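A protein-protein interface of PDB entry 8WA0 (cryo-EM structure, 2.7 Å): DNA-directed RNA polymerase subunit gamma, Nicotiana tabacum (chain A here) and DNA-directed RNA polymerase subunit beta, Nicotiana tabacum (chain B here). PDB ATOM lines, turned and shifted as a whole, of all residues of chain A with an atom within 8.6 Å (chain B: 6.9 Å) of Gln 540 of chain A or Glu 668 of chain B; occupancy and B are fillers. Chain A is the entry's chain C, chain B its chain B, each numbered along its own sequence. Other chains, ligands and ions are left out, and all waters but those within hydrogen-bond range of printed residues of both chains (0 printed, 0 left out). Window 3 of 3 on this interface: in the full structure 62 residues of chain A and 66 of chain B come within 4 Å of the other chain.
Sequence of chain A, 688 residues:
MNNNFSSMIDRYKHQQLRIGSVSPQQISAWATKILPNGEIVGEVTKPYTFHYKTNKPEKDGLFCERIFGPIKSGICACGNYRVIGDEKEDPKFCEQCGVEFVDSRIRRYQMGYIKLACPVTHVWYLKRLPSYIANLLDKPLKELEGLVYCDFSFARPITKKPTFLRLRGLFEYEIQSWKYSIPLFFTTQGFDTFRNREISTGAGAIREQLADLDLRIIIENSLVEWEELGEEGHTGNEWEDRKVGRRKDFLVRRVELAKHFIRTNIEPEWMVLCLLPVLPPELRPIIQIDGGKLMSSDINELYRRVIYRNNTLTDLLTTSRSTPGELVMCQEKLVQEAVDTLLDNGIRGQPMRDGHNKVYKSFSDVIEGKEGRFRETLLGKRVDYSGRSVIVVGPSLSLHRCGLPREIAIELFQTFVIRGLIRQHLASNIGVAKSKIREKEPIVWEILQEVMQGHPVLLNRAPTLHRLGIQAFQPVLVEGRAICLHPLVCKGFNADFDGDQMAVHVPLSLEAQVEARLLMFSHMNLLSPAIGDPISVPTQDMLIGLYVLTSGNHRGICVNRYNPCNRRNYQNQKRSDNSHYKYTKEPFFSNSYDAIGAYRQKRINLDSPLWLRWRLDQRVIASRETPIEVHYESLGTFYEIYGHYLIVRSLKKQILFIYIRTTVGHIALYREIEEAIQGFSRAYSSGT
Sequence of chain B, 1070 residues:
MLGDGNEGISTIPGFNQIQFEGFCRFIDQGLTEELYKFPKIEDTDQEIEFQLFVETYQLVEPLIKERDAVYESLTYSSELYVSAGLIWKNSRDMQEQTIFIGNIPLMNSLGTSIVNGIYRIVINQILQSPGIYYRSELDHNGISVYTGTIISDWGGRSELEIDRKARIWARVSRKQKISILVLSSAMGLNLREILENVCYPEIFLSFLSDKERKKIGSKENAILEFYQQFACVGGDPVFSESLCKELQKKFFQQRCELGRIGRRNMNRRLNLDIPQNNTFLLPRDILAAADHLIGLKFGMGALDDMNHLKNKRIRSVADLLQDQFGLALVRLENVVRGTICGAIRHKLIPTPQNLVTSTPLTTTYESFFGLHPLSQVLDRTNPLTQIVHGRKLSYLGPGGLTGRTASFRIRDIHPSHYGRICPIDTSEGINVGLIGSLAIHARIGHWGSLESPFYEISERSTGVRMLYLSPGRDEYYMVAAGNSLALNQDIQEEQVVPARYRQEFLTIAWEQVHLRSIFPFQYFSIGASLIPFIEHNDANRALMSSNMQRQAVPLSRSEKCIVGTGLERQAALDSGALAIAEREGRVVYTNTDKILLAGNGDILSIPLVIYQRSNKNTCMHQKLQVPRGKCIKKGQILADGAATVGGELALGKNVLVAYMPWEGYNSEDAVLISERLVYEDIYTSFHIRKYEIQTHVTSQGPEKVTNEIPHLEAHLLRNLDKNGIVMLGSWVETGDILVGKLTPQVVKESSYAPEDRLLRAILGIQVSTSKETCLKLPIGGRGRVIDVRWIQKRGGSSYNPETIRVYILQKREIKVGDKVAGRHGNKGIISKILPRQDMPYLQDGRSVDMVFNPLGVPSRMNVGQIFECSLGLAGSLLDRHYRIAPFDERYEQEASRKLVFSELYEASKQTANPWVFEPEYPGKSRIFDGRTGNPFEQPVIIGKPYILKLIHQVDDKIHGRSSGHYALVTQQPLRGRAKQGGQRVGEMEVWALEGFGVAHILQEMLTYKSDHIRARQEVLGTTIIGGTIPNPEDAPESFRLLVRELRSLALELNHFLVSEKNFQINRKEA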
ATOM      1  N   VAL A 392     -21.700 -19.710 -22.778  1.00  0.00           N
ATOM      2  CA  VAL A 392     -20.392 -19.041 -22.821  1.00  0.00           C
ATOM      3  C   VAL A 392     -20.418 -17.801 -23.700  1.00  0.00           C
ATOM      4  O   VAL A 392     -21.345 -17.634 -24.466  1.00  0.00           O
ATOM      5  CB  VAL A 392     -19.248 -19.966 -23.236  1.00  0.00           C
ATOM      6  CG1 VAL A 392     -18.864 -20.902 -22.107  1.00  0.00           C
ATOM      7  CG2 VAL A 392     -19.597 -20.733 -24.491  1.00  0.00           C
ATOM      8  N   VAL A 393     -19.416 -16.932 -23.610  1.00  0.00           N
ATOM      9  CA  VAL A 393     -19.428 -15.637 -24.313  1.00  0.00           C
ATOM     10  C   VAL A 393     -19.484 -15.485 -25.815  1.00  0.00           C
ATOM     11  O   VAL A 393     -20.082 -14.536 -26.265  1.00  0.00           O
ATOM     12  CB  VAL A 393     -18.278 -14.740 -23.852  1.00  0.00           C
ATOM     13  N   HIS A 486     -24.208 -14.424 -28.410  1.00  0.00           N
ATOM     14  CA  HIS A 486     -23.694 -13.111 -28.777  1.00  0.00           C
ATOM     15  C   HIS A 486     -23.661 -12.207 -27.577  1.00  0.00           C
ATOM     16  O   HIS A 486     -24.514 -12.280 -26.721  1.00  0.00           O
ATOM     17  CB  HIS A 486     -24.625 -12.499 -29.813  1.00  0.00           C
ATOM     18  CG  HIS A 486     -24.075 -11.297 -30.507  1.00  0.00           C
ATOM     19  ND1 HIS A 486     -24.313 -10.012 -30.077  1.00  0.00           N
ATOM     20  CD2 HIS A 486     -23.311 -11.184 -31.617  1.00  0.00           C
ATOM     21  CE1 HIS A 486     -23.710  -9.159 -30.884  1.00  0.00           C
ATOM     22  NE2 HIS A 486     -23.095  -9.846 -31.828  1.00  0.00           N
ATOM     23  N   PRO A 487     -22.666 -11.338 -27.504  1.00  0.00           N
ATOM     24  CA  PRO A 487     -22.554 -10.484 -26.333  1.00  0.00           C
ATOM     25  C   PRO A 487     -23.747  -9.557 -26.101  1.00  0.00           C
ATOM     26  O   PRO A 487     -24.109  -9.361 -24.956  1.00  0.00           O
ATOM     27  CB  PRO A 487     -21.310  -9.684 -26.640  1.00  0.00           C
ATOM     28  CG  PRO A 487     -20.463 -10.608 -27.426  1.00  0.00           C
ATOM     29  CD  PRO A 487     -21.424 -11.354 -28.294  1.00  0.00           C
ATOM     30  N   LEU A 488     -24.353  -8.996 -27.134  1.00  0.00           N
ATOM     31  CA  LEU A 488     -25.431  -8.017 -26.969  1.00  0.00           C
ATOM     32  C   LEU A 488     -26.844  -8.505 -26.671  1.00  0.00           C
ATOM     33  O   LEU A 488     -27.729  -7.692 -26.473  1.00  0.00           O
ATOM     34  CB  LEU A 488     -25.475  -7.126 -28.200  1.00  0.00           C
ATOM     35  CG  LEU A 488     -24.255  -6.257 -28.477  1.00  0.00           C
ATOM     36  CD1 LEU A 488     -24.384  -5.589 -29.833  1.00  0.00           C
ATOM     37  CD2 LEU A 488     -24.111  -5.221 -27.381  1.00  0.00           C
ATOM     38  N   CYS A 490     -27.518 -10.517 -24.120  1.00  0.00           N
ATOM     39  CA  CYS A 490     -27.556 -10.872 -22.717  1.00  0.00           C
ATOM     40  C   CYS A 490     -28.435 -10.018 -21.822  1.00  0.00           C
ATOM     41  O   CYS A 490     -28.916 -10.508 -20.821  1.00  0.00           O
ATOM     42  CB  CYS A 490     -26.146 -10.872 -22.161  1.00  0.00           C
ATOM     43  SG  CYS A 490     -25.066 -12.091 -22.927  1.00  0.00           S
ATOM     44  N   LYS A 491     -28.648  -8.755 -22.140  1.00  0.00           N
ATOM     45  CA  LYS A 491     -29.544  -7.969 -21.313  1.00  0.00           C
ATOM     46  C   LYS A 491     -30.954  -8.478 -21.334  1.00  0.00           C
ATOM     47  O   LYS A 491     -31.607  -8.516 -20.303  1.00  0.00           O
ATOM     48  CB  LYS A 491     -29.562  -6.509 -21.728  1.00  0.00           C
ATOM     49  CG  LYS A 491     -28.346  -5.709 -21.307  1.00  0.00           C
ATOM     50  CD  LYS A 491     -28.592  -4.224 -21.519  1.00  0.00           C
ATOM     51  CE  LYS A 491     -27.335  -3.401 -21.282  1.00  0.00           C
ATOM     52  NZ  LYS A 491     -26.754  -3.621 -19.928  1.00  0.00           N
ATOM     53  N   ASN A 494     -31.187 -11.424 -19.451  1.00  0.00           N
ATOM     54  CA  ASN A 494     -30.659 -11.214 -18.098  1.00  0.00           C
ATOM     55  C   ASN A 494     -29.628 -12.259 -17.765  1.00  0.00           C
ATOM     56  O   ASN A 494     -29.657 -12.838 -16.689  1.00  0.00           O
ATOM     57  CB  ASN A 494     -31.763 -11.159 -17.052  1.00  0.00           C
ATOM     58  N   ALA A 495     -28.705 -12.499 -18.682  1.00  0.00           N
ATOM     59  CA  ALA A 495     -27.727 -13.559 -18.496  1.00  0.00           C
ATOM     60  C   ALA A 495     -26.318 -13.108 -18.233  1.00  0.00           C
ATOM     61  O   ALA A 495     -25.882 -12.088 -18.749  1.00  0.00           O
ATOM     62  CB  ALA A 495     -27.736 -14.455 -19.705  1.00  0.00           C
ATOM     63  N   ASP A 496     -25.602 -13.860 -17.414  1.00  0.00           N
ATOM     64  CA  ASP A 496     -24.218 -13.557 -17.113  1.00  0.00           C
ATOM     65  C   ASP A 496     -23.511 -14.864 -17.297  1.00  0.00           C
ATOM     66  O   ASP A 496     -24.148 -15.899 -17.392  1.00  0.00           O
ATOM     67  CB  ASP A 496     -24.044 -13.068 -15.686  1.00  0.00           C
ATOM     68  CG  ASP A 496     -25.314 -13.174 -14.867  1.00  0.00           C
ATOM     69  OD1 ASP A 496     -26.228 -12.348 -15.071  1.00  0.00           O
ATOM     70  OD2 ASP A 496     -25.397 -14.068 -14.003  1.00  0.00           O
ATOM     71  N   PHE A 497     -22.198 -14.844 -17.336  1.00  0.00           N
ATOM     72  CA  PHE A 497     -21.491 -16.068 -17.615  1.00  0.00           C
ATOM     73  C   PHE A 497     -20.838 -16.677 -16.396  1.00  0.00           C
ATOM     74  O   PHE A 497     -19.670 -17.025 -16.426  1.00  0.00           O
ATOM     75  CB  PHE A 497     -20.532 -15.860 -18.777  1.00  0.00           C
ATOM     76  CG  PHE A 497     -21.214 -15.387 -20.022  1.00  0.00           C
ATOM     77  CD1 PHE A 497     -22.025 -16.240 -20.740  1.00  0.00           C
ATOM     78  CD2 PHE A 497     -21.077 -14.085 -20.452  1.00  0.00           C
ATOM     79  CE1 PHE A 497     -22.673 -15.810 -21.878  1.00  0.00           C
ATOM     80  CE2 PHE A 497     -21.723 -13.647 -21.586  1.00  0.00           C
ATOM     81  CZ  PHE A 497     -22.520 -14.512 -22.304  1.00  0.00           C
ATOM     82  N   ASP A 498     -21.605 -16.836 -15.330  1.00  0.00           N
ATOM     83  CA  ASP A 498     -21.089 -17.475 -14.140  1.00  0.00           C
ATOM     84  C   ASP A 498     -22.039 -18.543 -13.662  1.00  0.00           C
ATOM     85  O   ASP A 498     -22.596 -18.447 -12.580  1.00  0.00           O
ATOM     86  CB  ASP A 498     -20.859 -16.451 -13.043  1.00  0.00           C
ATOM     87  CG  ASP A 498     -21.995 -15.440 -12.911  1.00  0.00           C
ATOM     88  OD1 ASP A 498     -23.125 -15.705 -13.368  1.00  0.00           O
ATOM     89  OD2 ASP A 498     -21.751 -14.364 -12.331  1.00  0.00           O
ATOM     90  N   VAL A 537     -27.555  -2.379 -26.476  1.00  0.00           N
ATOM     91  CA  VAL A 537     -26.665  -1.266 -26.684  1.00  0.00           C
ATOM     92  C   VAL A 537     -25.320  -1.666 -26.129  1.00  0.00           C
ATOM     93  O   VAL A 537     -25.254  -2.538 -25.282  1.00  0.00           O
ATOM     94  CB  VAL A 537     -27.176  -0.033 -25.935  1.00  0.00           C
ATOM     95  N   PRO A 538     -24.233  -1.055 -26.611  1.00  0.00           N
ATOM     96  CA  PRO A 538     -22.954  -1.513 -26.093  1.00  0.00           C
ATOM     97  C   PRO A 538     -22.930  -1.320 -24.598  1.00  0.00           C
ATOM     98  O   PRO A 538     -23.354  -0.275 -24.140  1.00  0.00           O
ATOM     99  CB  PRO A 538     -21.990  -0.571 -26.767  1.00  0.00           C
ATOM    100  CG  PRO A 538     -22.609  -0.311 -28.091  1.00  0.00           C
ATOM    101  CD  PRO A 538     -24.075  -0.214 -27.806  1.00  0.00           C
ATOM    102  N   THR A 539     -22.446  -2.292 -23.832  1.00  0.00           N
ATOM    103  CA  THR A 539     -22.558  -2.184 -22.378  1.00  0.00           C
ATOM    104  C   THR A 539     -21.370  -2.089 -21.425  1.00  0.00           C
ATOM    105  O   THR A 539     -21.375  -1.226 -20.563  1.00  0.00           O
ATOM    106  CB  THR A 539     -23.536  -3.237 -21.832  1.00  0.00           C
ATOM    107  OG1 THR A 539     -23.484  -3.247 -20.403  1.00  0.00           O
ATOM    108  CG2 THR A 539     -23.197  -4.617 -22.360  1.00  0.00           C
ATOM    109  N   GLN A 540     -20.374  -2.950 -21.511  1.00  0.00           N
ATOM    110  CA  GLN A 540     -19.309  -2.866 -20.518  1.00  0.00           C
ATOM    111  C   GLN A 540     -17.948  -2.564 -21.085  1.00  0.00           C
ATOM    112  O   GLN A 540     -17.549  -1.415 -21.164  1.00  0.00           O
ATOM    113  CB  GLN A 540     -19.246  -4.132 -19.694  1.00  0.00           C
ATOM    114  CG  GLN A 540     -20.446  -4.353 -18.802  1.00  0.00           C
ATOM    115  CD  GLN A 540     -20.359  -5.661 -18.059  1.00  0.00           C
ATOM    116  OE1 GLN A 540     -19.358  -6.367 -18.148  1.00  0.00           O
ATOM    117  NE2 GLN A 540     -21.407  -5.993 -17.322  1.00  0.00           N
ATOM    118  N   ASP A 541     -17.226  -3.590 -21.485  1.00  0.00           N
ATOM    119  CA  ASP A 541     -15.918  -3.390 -22.067  1.00  0.00           C
ATOM    120  C   ASP A 541     -16.050  -2.616 -23.345  1.00  0.00           C
ATOM    121  O   ASP A 541     -15.203  -1.807 -23.670  1.00  0.00           O
ATOM    122  CB  ASP A 541     -15.220  -4.701 -22.356  1.00  0.00           C
ATOM    123  CG  ASP A 541     -15.126  -5.604 -21.143  1.00  0.00           C
ATOM    124  OD1 ASP A 541     -15.638  -5.233 -20.069  1.00  0.00           O
ATOM    125  OD2 ASP A 541     -14.534  -6.696 -21.267  1.00  0.00           O
ATOM    126  N   MET A 542     -17.099  -2.876 -24.096  1.00  0.00           N
ATOM    127  CA  MET A 542     -17.278  -2.201 -25.345  1.00  0.00           C
ATOM    128  C   MET A 542     -17.398  -0.731 -25.082  1.00  0.00           C
ATOM    129  O   MET A 542     -16.784   0.060 -25.762  1.00  0.00           O
ATOM    130  CB  MET A 542     -18.535  -2.693 -26.017  1.00  0.00           C
ATOM    131  CG  MET A 542     -18.743  -4.183 -25.877  1.00  0.00           C
ATOM    132  SD  MET A 542     -20.405  -4.703 -26.307  1.00  0.00           S
ATOM    133  CE  MET A 542     -20.623  -3.767 -27.806  1.00  0.00           C
ATOM    134  N   LEU A 543     -18.135  -0.353 -24.058  1.00  0.00           N
ATOM    135  CA  LEU A 543     -18.256   1.047 -23.722  1.00  0.00           C
ATOM    136  C   LEU A 543     -16.932   1.660 -23.327  1.00  0.00           C
ATOM    137  O   LEU A 543     -16.671   2.803 -23.655  1.00  0.00           O
ATOM    138  CB  LEU A 543     -19.299   1.280 -22.649  1.00  0.00           C
ATOM    139  CG  LEU A 543     -20.661   1.776 -23.107  1.00  0.00           C
ATOM    140  CD1 LEU A 543     -21.499   2.077 -21.880  1.00  0.00           C
ATOM    141  CD2 LEU A 543     -20.492   3.023 -23.956  1.00  0.00           C
ATOM    142  N   ILE A 544     -16.102   0.914 -22.622  1.00  0.00           N
ATOM    143  CA  ILE A 544     -14.803   1.421 -22.229  1.00  0.00           C
ATOM    144  C   ILE A 544     -14.032   1.802 -23.470  1.00  0.00           C
ATOM    145  O   ILE A 544     -13.466   2.878 -23.538  1.00  0.00           O
ATOM    146  CB  ILE A 544     -14.018   0.400 -21.396  1.00  0.00           C
ATOM    147  CG1 ILE A 544     -14.670   0.207 -20.036  1.00  0.00           C
ATOM    148  CG2 ILE A 544     -12.585   0.847 -21.187  1.00  0.00           C
ATOM    149  CD1 ILE A 544     -14.494   1.395 -19.124  1.00  0.00           C
ATOM    150  N   GLY A 545     -14.036   0.947 -24.473  1.00  0.00           N
ATOM    151  CA  GLY A 545     -13.299   1.227 -25.680  1.00  0.00           C
ATOM    152  C   GLY A 545     -13.774   2.439 -26.427  1.00  0.00           C
ATOM    153  O   GLY A 545     -12.969   3.224 -26.894  1.00  0.00           O
ATOM    154  N   LEU A 546     -15.075   2.614 -26.538  1.00  0.00           N
ATOM    155  CA  LEU A 546     -15.619   3.776 -27.206  1.00  0.00           C
ATOM    156  C   LEU A 546     -15.276   5.052 -26.482  1.00  0.00           C
ATOM    157  O   LEU A 546     -14.968   6.051 -27.106  1.00  0.00           O
ATOM    158  CB  LEU A 546     -17.118   3.640 -27.388  1.00  0.00           C
ATOM    159  N   TYR A 547     -15.320   5.031 -25.163  1.00  0.00           N
ATOM    160  CA  TYR A 547     -14.965   6.200 -24.390  1.00  0.00           C
ATOM    161  C   TYR A 547     -13.527   6.577 -24.600  1.00  0.00           C
ATOM    162  O   TYR A 547     -13.216   7.735 -24.761  1.00  0.00           O
ATOM    163  CB  TYR A 547     -15.196   5.941 -22.915  1.00  0.00           C
ATOM    164  CG  TYR A 547     -14.958   7.127 -22.021  1.00  0.00           C
ATOM    165  CD1 TYR A 547     -15.943   8.077 -21.828  1.00  0.00           C
ATOM    166  CD2 TYR A 547     -13.753   7.288 -21.356  1.00  0.00           C
ATOM    167  CE1 TYR A 547     -15.732   9.163 -21.008  1.00  0.00           C
ATOM    168  CE2 TYR A 547     -13.532   8.371 -20.536  1.00  0.00           C
ATOM    169  CZ  TYR A 547     -14.524   9.303 -20.365  1.00  0.00           C
ATOM    170  OH  TYR A 547     -14.307  10.382 -19.548  1.00  0.00           O
ATOM    171  N   GLY B 664     -12.977  -9.563 -25.773  1.00  0.00           N
ATOM    172  CA  GLY B 664     -14.331  -9.942 -25.451  1.00  0.00           C
ATOM    173  C   GLY B 664     -14.512 -11.314 -24.883  1.00  0.00           C
ATOM    174  O   GLY B 664     -15.596 -11.655 -24.458  1.00  0.00           O
ATOM    175  N   TYR B 665     -13.459 -12.106 -24.852  1.00  0.00           N
ATOM    176  CA  TYR B 665     -13.528 -13.419 -24.269  1.00  0.00           C
ATOM    177  C   TYR B 665     -13.793 -13.363 -22.793  1.00  0.00           C
ATOM    178  O   TYR B 665     -14.453 -14.230 -22.268  1.00  0.00           O
ATOM    179  CB  TYR B 665     -12.336 -14.245 -24.660  1.00  0.00           C
ATOM    180  CG  TYR B 665     -12.385 -14.616 -26.114  1.00  0.00           C
ATOM    181  CD1 TYR B 665     -13.210 -15.633 -26.554  1.00  0.00           C
ATOM    182  CD2 TYR B 665     -11.631 -13.934 -27.049  1.00  0.00           C
ATOM    183  CE1 TYR B 665     -13.274 -15.972 -27.886  1.00  0.00           C
ATOM    184  CE2 TYR B 665     -11.688 -14.265 -28.384  1.00  0.00           C
ATOM    185  CZ  TYR B 665     -12.511 -15.286 -28.795  1.00  0.00           C
ATOM    186  OH  TYR B 665     -12.572 -15.624 -30.122  1.00  0.00           O
ATOM    187  N   ASN B 666     -13.428 -12.269 -22.152  1.00  0.00           N
ATOM    188  CA  ASN B 666     -13.668 -12.090 -20.734  1.00  0.00           C
ATOM    189  C   ASN B 666     -14.906 -11.279 -20.414  1.00  0.00           C
ATOM    190  O   ASN B 666     -15.025 -10.798 -19.308  1.00  0.00           O
ATOM    191  CB  ASN B 666     -12.505 -11.330 -20.112  1.00  0.00           C
ATOM    192  CG  ASN B 666     -11.190 -12.039 -20.245  1.00  0.00           C
ATOM    193  OD1 ASN B 666     -10.146 -11.403 -20.270  1.00  0.00           O
ATOM    194  ND2 ASN B 666     -11.227 -13.357 -20.324  1.00  0.00           N
ATOM    195  N   SER B 667     -15.833 -11.112 -21.343  1.00  0.00           N
ATOM    196  CA  SER B 667     -16.993 -10.262 -21.094  1.00  0.00           C
ATOM    197  C   SER B 667     -17.805 -10.844 -19.998  1.00  0.00           C
ATOM    198  O   SER B 667     -17.847 -12.053 -19.853  1.00  0.00           O
ATOM    199  CB  SER B 667     -17.870 -10.103 -22.325  1.00  0.00           C
ATOM    200  OG  SER B 667     -18.909  -9.163 -22.115  1.00  0.00           O
ATOM    201  N   GLU B 668     -18.450  -9.999 -19.208  1.00  0.00           N
ATOM    202  CA  GLU B 668     -19.191 -10.471 -18.059  1.00  0.00           C
ATOM    203  C   GLU B 668     -18.177 -11.198 -17.231  1.00  0.00           C
ATOM    204  O   GLU B 668     -17.164 -10.616 -16.878  1.00  0.00           O
ATOM    205  CB  GLU B 668     -20.382 -11.322 -18.426  1.00  0.00           C
ATOM    206  CG  GLU B 668     -21.444 -10.578 -19.213  1.00  0.00           C
ATOM    207  CD  GLU B 668     -22.097  -9.469 -18.413  1.00  0.00           C
ATOM    208  OE1 GLU B 668     -22.267  -9.631 -17.188  1.00  0.00           O
ATOM    209  OE2 GLU B 668     -22.457  -8.438 -19.014  1.00  0.00           O
ATOM    210  N   ASP B 669     -18.399 -12.450 -16.898  1.00  0.00           N
ATOM    211  CA  ASP B 669     -17.446 -13.095 -16.038  1.00  0.00           C
ATOM    212  C   ASP B 669     -16.953 -14.339 -16.670  1.00  0.00           C
ATOM    213  O   ASP B 669     -17.358 -15.413 -16.296  1.00  0.00           O
ATOM    214  CB  ASP B 669     -18.114 -13.493 -14.753  1.00  0.00           C
ATOM    215  CG  ASP B 669     -18.506 -12.312 -13.909  1.00  0.00           C
ATOM    216  OD1 ASP B 669     -17.855 -11.258 -14.024  1.00  0.00           O
ATOM    217  OD2 ASP B 669     -19.460 -12.445 -13.116  1.00  0.00           O
ATOM    218  N   ALA B 670     -16.049 -14.211 -17.609  1.00  0.00           N
ATOM    219  CA  ALA B 670     -15.567 -15.361 -18.301  1.00  0.00           C
ATOM    220  C   ALA B 670     -14.073 -15.320 -18.296  1.00  0.00           C
ATOM    221  O   ALA B 670     -13.503 -14.261 -18.143  1.00  0.00           O
ATOM    222  CB  ALA B 670     -16.103 -15.348 -19.691  1.00  0.00           C
ATOM    223  N   ASN B 853     -11.165 -10.241 -16.205  1.00  0.00           N
ATOM    224  CA  ASN B 853     -11.672  -8.908 -16.489  1.00  0.00           C
ATOM    225  C   ASN B 853     -11.407  -7.970 -15.349  1.00  0.00           C
ATOM    226  O   ASN B 853     -11.517  -8.360 -14.204  1.00  0.00           O
ATOM    227  CB  ASN B 853     -13.170  -8.975 -16.695  1.00  0.00           C
ATOM    228  CG  ASN B 853     -13.696  -7.864 -17.571  1.00  0.00           C
ATOM    229  OD1 ASN B 853     -14.706  -7.246 -17.257  1.00  0.00           O
ATOM    230  ND2 ASN B 853     -13.017  -7.609 -18.678  1.00  0.00           N
ATOM    231  N   LEU B 855     -13.111  -5.151 -14.667  1.00  0.00           N
ATOM    232  CA  LEU B 855     -14.230  -4.291 -14.382  1.00  0.00           C
ATOM    233  C   LEU B 855     -15.028  -4.865 -13.334  1.00  0.00           C
ATOM    234  O   LEU B 855     -15.896  -4.242 -12.778  1.00  0.00           O
ATOM    235  CB  LEU B 855     -15.089  -4.066 -15.622  1.00  0.00           C
ATOM    236  CG  LEU B 855     -14.623  -2.955 -16.546  1.00  0.00           C
ATOM    237  CD1 LEU B 855     -13.736  -3.477 -17.656  1.00  0.00           C
ATOM    238  CD2 LEU B 855     -15.840  -2.295 -17.133  1.00  0.00           C
ATOM    239  N   GLY B 856     -14.649  -6.059 -12.919  1.00  0.00           N
ATOM    240  CA  GLY B 856     -15.359  -6.732 -11.852  1.00  0.00           C
ATOM    241  C   GLY B 856     -15.169  -6.219 -10.441  1.00  0.00           C
ATOM    242  O   GLY B 856     -16.121  -6.165  -9.680  1.00  0.00           O
ATOM    243  N   ARG B 860     -18.062  -5.465  -7.409  1.00  0.00           N
ATOM    244  CA  ARG B 860     -18.160  -6.443  -6.337  1.00  0.00           C
ATOM    245  C   ARG B 860     -17.424  -6.106  -5.063  1.00  0.00           C
ATOM    246  O   ARG B 860     -17.537  -6.832  -4.099  1.00  0.00           O
ATOM    247  CB  ARG B 860     -17.754  -7.807  -6.850  1.00  0.00           C
ATOM    248  CG  ARG B 860     -18.852  -8.493  -7.630  1.00  0.00           C
ATOM    249  CD  ARG B 860     -18.398  -8.847  -9.030  1.00  0.00           C
ATOM    250  NE  ARG B 860     -19.522  -9.271  -9.853  1.00  0.00           N
ATOM    251  CZ  ARG B 860     -19.420  -9.604 -11.132  1.00  0.00           C
ATOM    252  NH1 ARG B 860     -18.243  -9.561 -11.736  1.00  0.00           N
ATOM    253  NH2 ARG B 860     -20.495  -9.978 -11.808  1.00  0.00           N
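The backbone carbonyl oxygen (O) of Phe 497 of chain A lies close to the backbone carbonyl oxygen (O) of Asp 669 of chain B, at 2.8 Å. The side-chain carboxylate (OD2) of Asp 541 of chain A is in hydrogen-bond range of the side-chain amide nitrogen (ND2) of Asn 853 of chain B (3.1 Å). OD2 of Asp 498 of chain A lies close to OD2 of Asp 669 of chain B (3.1 Å). NE2 of Gln 540 of chain A lies within hydrogen-bond range of OE2 of Glu 668 of chain B, 3.2 Å away.
The guanidinium group (NH1) of Arg 860 of chain B is in salt-bridge range of the side-chain carboxylate (OD1) of Asp 669 of chain B (2.9 Å).
Phe 497 of chain A touches Ser 667 of chain B (CD2 to O, 3.9 Å). Phe 497 of chain A touches Glu 668 of chain B (CD2 to CB, 3.5 Å). Asp 541 of chain A touches Leu 855 of chain B (OD1 to CD1, 3.5 Å).
Glu 668 of chain B touches just these residues of chain A: Phe 497 (3.5 Å) and Gln 540 (3.2 Å). Asp 669 of chain B touches two residues of chain A. Of the printed residues of chain B, Phe 497 of chain A touches Ser 667 (3.9 Å), Glu 668 (3.5 Å) and Asp 669 (2.8 Å). Printed residues of chain A within 4 Å of Leu 855 of chain B: Asp 541 (3.5 Å). Of the printed residues of chain B, Asp 541 of chain A touches Asn 853 and Leu 855. Of the printed residues of chain B, Asp 498 of chain A touches Asp 669 (3.1 Å). The nearest residue of chain A that does not touch Glu 668 of chain B is Asp 496 of chain A (4.2 Å). The nearest printed residue of chain B that does not touch Asp 498 of chain A is Arg 860 of chain B (4.6 Å).
Printed residues of chain B that touch a printed residue of chain A: Ser 667, Glu 668, Asp 669, Asn 853 and Leu 855. Of the 23 printed residues of chain A, 4 touch a printed residue of chain B. Printed residues of chain A that touch a printed residue of chain B: Phe 497, Asp 498, Gln 540 and Asp 541. Hydrophobic or aromatic side chains of chain A that line the printed part of chain B: Phe 497.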
